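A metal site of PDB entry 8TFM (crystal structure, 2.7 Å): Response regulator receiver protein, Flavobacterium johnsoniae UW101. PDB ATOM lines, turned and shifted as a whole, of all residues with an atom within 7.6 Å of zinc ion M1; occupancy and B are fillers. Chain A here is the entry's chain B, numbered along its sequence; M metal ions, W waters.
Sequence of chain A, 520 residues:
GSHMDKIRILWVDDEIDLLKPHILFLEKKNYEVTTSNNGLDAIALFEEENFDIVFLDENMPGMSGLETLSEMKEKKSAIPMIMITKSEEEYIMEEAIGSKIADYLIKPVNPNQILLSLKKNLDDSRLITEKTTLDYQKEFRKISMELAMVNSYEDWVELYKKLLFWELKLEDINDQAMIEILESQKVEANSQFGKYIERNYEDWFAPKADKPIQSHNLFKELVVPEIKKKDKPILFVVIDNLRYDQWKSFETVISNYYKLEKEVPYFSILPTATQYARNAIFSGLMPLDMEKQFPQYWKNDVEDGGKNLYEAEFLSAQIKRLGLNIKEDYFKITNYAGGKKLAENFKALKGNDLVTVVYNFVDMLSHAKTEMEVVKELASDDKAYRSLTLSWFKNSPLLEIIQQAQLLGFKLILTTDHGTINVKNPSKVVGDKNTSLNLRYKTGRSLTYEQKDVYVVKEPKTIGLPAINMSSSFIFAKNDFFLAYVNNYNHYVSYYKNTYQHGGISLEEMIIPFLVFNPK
Of the 19 residues printed, 3 come within 4 Å of zinc ion M1.
The nearest printed residue that does not touch zinc ion M1 is Thr 274 (4.5 Å).
The side-chain carboxylate (OD1) of Asp 363 sits close to the side-chain amide nitrogen (ND2) of Asn 241.
O of Asp 363 lies within hydrogen-bond range of OG of Ser 366 (2.7 Å).
The backbone carbonyl oxygen (O) of His 502 is in hydrogen-bond range of the side-chain amide nitrogen (ND2) of Asn 438 (2.7 Å).
A ring nitrogen (ND1) of His 502 lies within hydrogen-bond range of the backbone carbonyl oxygen (O) of Thr 272 (2.9 Å).
Zinc ion M1 is bound by the side-chain carboxylate of Asp 363 (2.0 Å), a ring nitrogen (NE2) of His 367 (2.2 Å), a ring nitrogen (NE2) of His 502 (2.3 Å) and water W1 (2.6 Å).
Zinc ion M1 has four donor atoms within binding distance.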
ATOM      1  N   ASP A 240     -19.610  20.161 -22.305  1.00  0.00           N
ATOM      2  CA  ASP A 240     -20.141  20.165 -20.959  1.00  0.00           C
ATOM      3  C   ASP A 240     -19.459  19.069 -20.147  1.00  0.00           C
ATOM      4  O   ASP A 240     -19.311  17.950 -20.626  1.00  0.00           O
ATOM      5  CB  ASP A 240     -21.653  19.967 -20.956  1.00  0.00           C
ATOM      6  CG  ASP A 240     -22.304  20.520 -19.698  1.00  0.00           C
ATOM      7  OD1 ASP A 240     -22.560  21.720 -19.694  1.00  0.00           O
ATOM      8  OD2 ASP A 240     -22.457  19.741 -18.719  1.00  0.00           O
ATOM      9  N   ASN A 241     -19.072  19.403 -18.919  1.00  0.00           N
ATOM     10  CA  ASN A 241     -18.712  18.434 -17.906  1.00  0.00           C
ATOM     11  C   ASN A 241     -17.454  17.666 -18.326  1.00  0.00           C
ATOM     12  O   ASN A 241     -17.449  16.438 -18.299  1.00  0.00           O
ATOM     13  CB  ASN A 241     -19.880  17.481 -17.607  1.00  0.00           C
ATOM     14  CG  ASN A 241     -19.616  16.570 -16.414  1.00  0.00           C
ATOM     15  OD1 ASN A 241     -18.557  16.627 -15.807  1.00  0.00           O
ATOM     16  ND2 ASN A 241     -20.558  15.690 -16.093  1.00  0.00           N
ATOM     17  N   THR A 272     -20.647  24.048  -9.127  1.00  0.00           N
ATOM     18  CA  THR A 272     -20.058  23.532 -10.348  1.00  0.00           C
ATOM     19  C   THR A 272     -21.125  22.757 -11.143  1.00  0.00           C
ATOM     20  O   THR A 272     -20.998  21.554 -11.353  1.00  0.00           O
ATOM     21  CB  THR A 272     -18.817  22.671 -10.028  1.00  0.00           C
ATOM     22  OG1 THR A 272     -19.142  21.725  -9.010  1.00  0.00           O
ATOM     23  CG2 THR A 272     -17.644  23.493  -9.561  1.00  0.00           C
ATOM     24  N   ALA A 273     -22.182  23.488 -11.538  1.00  0.00           N
ATOM     25  CA  ALA A 273     -23.293  22.927 -12.292  1.00  0.00           C
ATOM     26  C   ALA A 273     -23.602  23.800 -13.512  1.00  0.00           C
ATOM     27  O   ALA A 273     -23.363  25.020 -13.492  1.00  0.00           O
ATOM     28  CB  ALA A 273     -24.507  22.799 -11.413  1.00  0.00           C
ATOM     29  N   THR A 274     -24.142  23.148 -14.552  1.00  0.00           N
ATOM     30  CA  THR A 274     -24.433  23.774 -15.838  1.00  0.00           C
ATOM     31  C   THR A 274     -25.239  25.062 -15.638  1.00  0.00           C
ATOM     32  O   THR A 274     -24.871  26.102 -16.192  1.00  0.00           O
ATOM     33  CB  THR A 274     -25.126  22.768 -16.772  1.00  0.00           C
ATOM     34  OG1 THR A 274     -24.382  21.538 -16.753  1.00  0.00           O
ATOM     35  CG2 THR A 274     -25.262  23.281 -18.197  1.00  0.00           C
ATOM     36  N   ASN A 360     -23.323  18.379 -25.190  1.00  0.00           N
ATOM     37  CA  ASN A 360     -23.812  17.944 -23.894  1.00  0.00           C
ATOM     38  C   ASN A 360     -23.581  16.444 -23.669  1.00  0.00           C
ATOM     39  O   ASN A 360     -23.984  15.895 -22.657  1.00  0.00           O
ATOM     40  CB  ASN A 360     -25.299  18.240 -23.743  1.00  0.00           C
ATOM     41  CG  ASN A 360     -25.631  19.674 -23.353  1.00  0.00           C
ATOM     42  OD1 ASN A 360     -24.746  20.480 -23.083  1.00  0.00           O
ATOM     43  ND2 ASN A 360     -26.918  19.993 -23.298  1.00  0.00           N
ATOM     44  N   VAL A 362     -21.045  14.543 -22.970  1.00  0.00           N
ATOM     45  CA  VAL A 362     -20.199  13.953 -21.943  1.00  0.00           C
ATOM     46  C   VAL A 362     -20.948  13.978 -20.610  1.00  0.00           C
ATOM     47  O   VAL A 362     -20.818  13.056 -19.803  1.00  0.00           O
ATOM     48  CB  VAL A 362     -18.842  14.669 -21.875  1.00  0.00           C
ATOM     49  CG1 VAL A 362     -17.961  14.079 -20.787  1.00  0.00           C
ATOM     50  CG2 VAL A 362     -18.113  14.640 -23.221  1.00  0.00           C
ATOM     51  N   ASP A 363     -21.758  15.011 -20.399  1.00  0.00           N
ATOM     52  CA  ASP A 363     -22.587  15.092 -19.210  1.00  0.00           C
ATOM     53  C   ASP A 363     -23.588  13.950 -19.189  1.00  0.00           C
ATOM     54  O   ASP A 363     -23.754  13.308 -18.161  1.00  0.00           O
ATOM     55  CB  ASP A 363     -23.300  16.446 -19.114  1.00  0.00           C
ATOM     56  CG  ASP A 363     -24.222  16.500 -17.916  1.00  0.00           C
ATOM     57  OD1 ASP A 363     -23.710  16.630 -16.768  1.00  0.00           O
ATOM     58  OD2 ASP A 363     -25.457  16.352 -18.133  1.00  0.00           O
ATOM     59  N   MET A 364     -24.254  13.698 -20.322  1.00  0.00           N
ATOM     60  CA  MET A 364     -25.222  12.631 -20.453  1.00  0.00           C
ATOM     61  C   MET A 364     -24.546  11.305 -20.110  1.00  0.00           C
ATOM     62  O   MET A 364     -25.113  10.494 -19.369  1.00  0.00           O
ATOM     63  CB  MET A 364     -25.767  12.551 -21.894  1.00  0.00           C
ATOM     64  CG  MET A 364     -27.112  13.265 -22.114  1.00  0.00           C
ATOM     65  SD  MET A 364     -27.265  13.854 -23.847  1.00  0.00           S
ATOM     66  CE  MET A 364     -28.268  15.320 -23.591  1.00  0.00           C
ATOM     67  N   SER A 366     -21.700  10.773 -18.347  1.00  0.00           N
ATOM     68  CA  SER A 366     -21.271  10.712 -16.960  1.00  0.00           C
ATOM     69  C   SER A 366     -22.449  10.322 -16.080  1.00  0.00           C
ATOM     70  O   SER A 366     -22.283   9.488 -15.188  1.00  0.00           O
ATOM     71  CB  SER A 366     -20.654  12.012 -16.498  1.00  0.00           C
ATOM     72  OG  SER A 366     -21.606  13.057 -16.484  1.00  0.00           O
ATOM     73  N   HIS A 367     -23.623  10.912 -16.358  1.00  0.00           N
ATOM     74  CA  HIS A 367     -24.840  10.660 -15.586  1.00  0.00           C
ATOM     75  C   HIS A 367     -25.386   9.267 -15.872  1.00  0.00           C
ATOM     76  O   HIS A 367     -26.106   8.713 -15.074  1.00  0.00           O
ATOM     77  CB  HIS A 367     -25.872  11.766 -15.829  1.00  0.00           C
ATOM     78  CG  HIS A 367     -25.468  13.071 -15.226  1.00  0.00           C
ATOM     79  ND1 HIS A 367     -25.279  13.288 -13.871  1.00  0.00           N
ATOM     80  CD2 HIS A 367     -25.197  14.234 -15.827  1.00  0.00           C
ATOM     81  CE1 HIS A 367     -24.919  14.555 -13.690  1.00  0.00           C
ATOM     82  NE2 HIS A 367     -24.842  15.137 -14.874  1.00  0.00           N
ATOM     83  N   ASP A 417     -17.630  23.776 -18.715  1.00  0.00           N
ATOM     84  CA  ASP A 417     -18.281  24.555 -17.673  1.00  0.00           C
ATOM     85  C   ASP A 417     -17.754  24.120 -16.308  1.00  0.00           C
ATOM     86  O   ASP A 417     -17.640  24.965 -15.412  1.00  0.00           O
ATOM     87  CB  ASP A 417     -19.811  24.485 -17.800  1.00  0.00           C
ATOM     88  CG  ASP A 417     -20.425  23.092 -17.792  1.00  0.00           C
ATOM     89  OD1 ASP A 417     -19.668  22.110 -18.049  1.00  0.00           O
ATOM     90  OD2 ASP A 417     -21.660  23.004 -17.506  1.00  0.00           O
ATOM     91  N   HIS A 418     -17.424  22.824 -16.171  1.00  0.00           N
ATOM     92  CA  HIS A 418     -17.003  22.210 -14.925  1.00  0.00           C
ATOM     93  C   HIS A 418     -16.699  20.740 -15.182  1.00  0.00           C
ATOM     94  O   HIS A 418     -17.038  20.244 -16.243  1.00  0.00           O
ATOM     95  CB  HIS A 418     -18.117  22.257 -13.869  1.00  0.00           C
ATOM     96  CG  HIS A 418     -19.344  21.604 -14.386  1.00  0.00           C
ATOM     97  ND1 HIS A 418     -19.452  20.230 -14.493  1.00  0.00           N
ATOM     98  CD2 HIS A 418     -20.472  22.121 -14.855  1.00  0.00           C
ATOM     99  CE1 HIS A 418     -20.637  19.938 -15.014  1.00  0.00           C
ATOM    100  NE2 HIS A 418     -21.261  21.066 -15.243  1.00  0.00           N
ATOM    101  N   GLY A 419     -16.072  20.060 -14.217  1.00  0.00           N
ATOM    102  CA  GLY A 419     -15.808  18.627 -14.292  1.00  0.00           C
ATOM    103  C   GLY A 419     -16.825  17.847 -13.480  1.00  0.00           C
ATOM    104  O   GLY A 419     -17.854  18.394 -13.093  1.00  0.00           O
ATOM    105  N   THR A 420     -16.557  16.549 -13.233  1.00  0.00           N
ATOM    106  CA  THR A 420     -17.386  15.718 -12.376  1.00  0.00           C
ATOM    107  C   THR A 420     -16.455  14.826 -11.535  1.00  0.00           C
ATOM    108  O   THR A 420     -15.345  14.567 -11.977  1.00  0.00           O
ATOM    109  CB  THR A 420     -18.365  14.875 -13.201  1.00  0.00           C
ATOM    110  OG1 THR A 420     -19.179  14.128 -12.294  1.00  0.00           O
ATOM    111  CG2 THR A 420     -17.672  13.894 -14.101  1.00  0.00           C
ATOM    112  N   ASN A 438     -29.586  18.345  -6.793  1.00  0.00           N
ATOM    113  CA  ASN A 438     -28.251  17.813  -7.059  1.00  0.00           C
ATOM    114  C   ASN A 438     -27.781  16.960  -5.871  1.00  0.00           C
ATOM    115  O   ASN A 438     -28.527  16.748  -4.922  1.00  0.00           O
ATOM    116  CB  ASN A 438     -27.331  18.979  -7.442  1.00  0.00           C
ATOM    117  CG  ASN A 438     -25.911  18.529  -7.750  1.00  0.00           C
ATOM    118  OD1 ASN A 438     -25.708  17.508  -8.401  1.00  0.00           O
ATOM    119  ND2 ASN A 438     -24.914  19.220  -7.214  1.00  0.00           N
ATOM    120  N   TYR A 500     -20.769   9.604 -11.028  1.00  0.00           N
ATOM    121  CA  TYR A 500     -20.171  10.892 -11.312  1.00  0.00           C
ATOM    122  C   TYR A 500     -21.208  11.967 -10.971  1.00  0.00           C
ATOM    123  O   TYR A 500     -22.296  11.957 -11.534  1.00  0.00           O
ATOM    124  CB  TYR A 500     -19.645  10.926 -12.762  1.00  0.00           C
ATOM    125  CG  TYR A 500     -18.465  10.003 -13.029  1.00  0.00           C
ATOM    126  CD1 TYR A 500     -17.228  10.267 -12.459  1.00  0.00           C
ATOM    127  CD2 TYR A 500     -18.598   8.840 -13.780  1.00  0.00           C
ATOM    128  CE1 TYR A 500     -16.140   9.426 -12.669  1.00  0.00           C
ATOM    129  CE2 TYR A 500     -17.515   8.011 -14.008  1.00  0.00           C
ATOM    130  CZ  TYR A 500     -16.290   8.281 -13.420  1.00  0.00           C
ATOM    131  OH  TYR A 500     -15.177   7.487 -13.579  1.00  0.00           O
ATOM    132  N   GLN A 501     -20.886  12.861 -10.025  1.00  0.00           N
ATOM    133  CA  GLN A 501     -21.745  13.985  -9.665  1.00  0.00           C
ATOM    134  C   GLN A 501     -20.936  15.265  -9.762  1.00  0.00           C
ATOM    135  O   GLN A 501     -19.721  15.208  -9.688  1.00  0.00           O
ATOM    136  CB  GLN A 501     -22.228  13.912  -8.219  1.00  0.00           C
ATOM    137  CG  GLN A 501     -23.019  12.660  -7.890  1.00  0.00           C
ATOM    138  CD  GLN A 501     -24.233  12.510  -8.771  1.00  0.00           C
ATOM    139  OE1 GLN A 501     -24.895  13.485  -9.125  1.00  0.00           O
ATOM    140  NE2 GLN A 501     -24.530  11.263  -9.115  1.00  0.00           N
ATOM    141  N   HIS A 502     -21.595  16.422  -9.901  1.00  0.00           N
ATOM    142  CA  HIS A 502     -20.897  17.686  -9.901  1.00  0.00           C
ATOM    143  C   HIS A 502     -21.734  18.746  -9.189  1.00  0.00           C
ATOM    144  O   HIS A 502     -22.844  18.467  -8.732  1.00  0.00           O
ATOM    145  CB  HIS A 502     -20.521  18.083 -11.327  1.00  0.00           C
ATOM    146  CG  HIS A 502     -21.704  18.145 -12.227  1.00  0.00           C
ATOM    147  ND1 HIS A 502     -22.467  19.282 -12.317  1.00  0.00           N
ATOM    148  CD2 HIS A 502     -22.165  17.276 -13.133  1.00  0.00           C
ATOM    149  CE1 HIS A 502     -23.392  19.101 -13.245  1.00  0.00           C
ATOM    150  NE2 HIS A 502     -23.237  17.892 -13.752  1.00  0.00           N
HETATM  151 ZN    ZN M   1     -24.829  17.296 -15.273  1.00  0.00          ZN
HETATM  152 ZN    ZN M   2     -22.379  21.558 -17.252  1.00  0.00          ZN
HETATM  153  O   HOH W   1     -26.111  19.429 -15.854  1.00  0.00           O
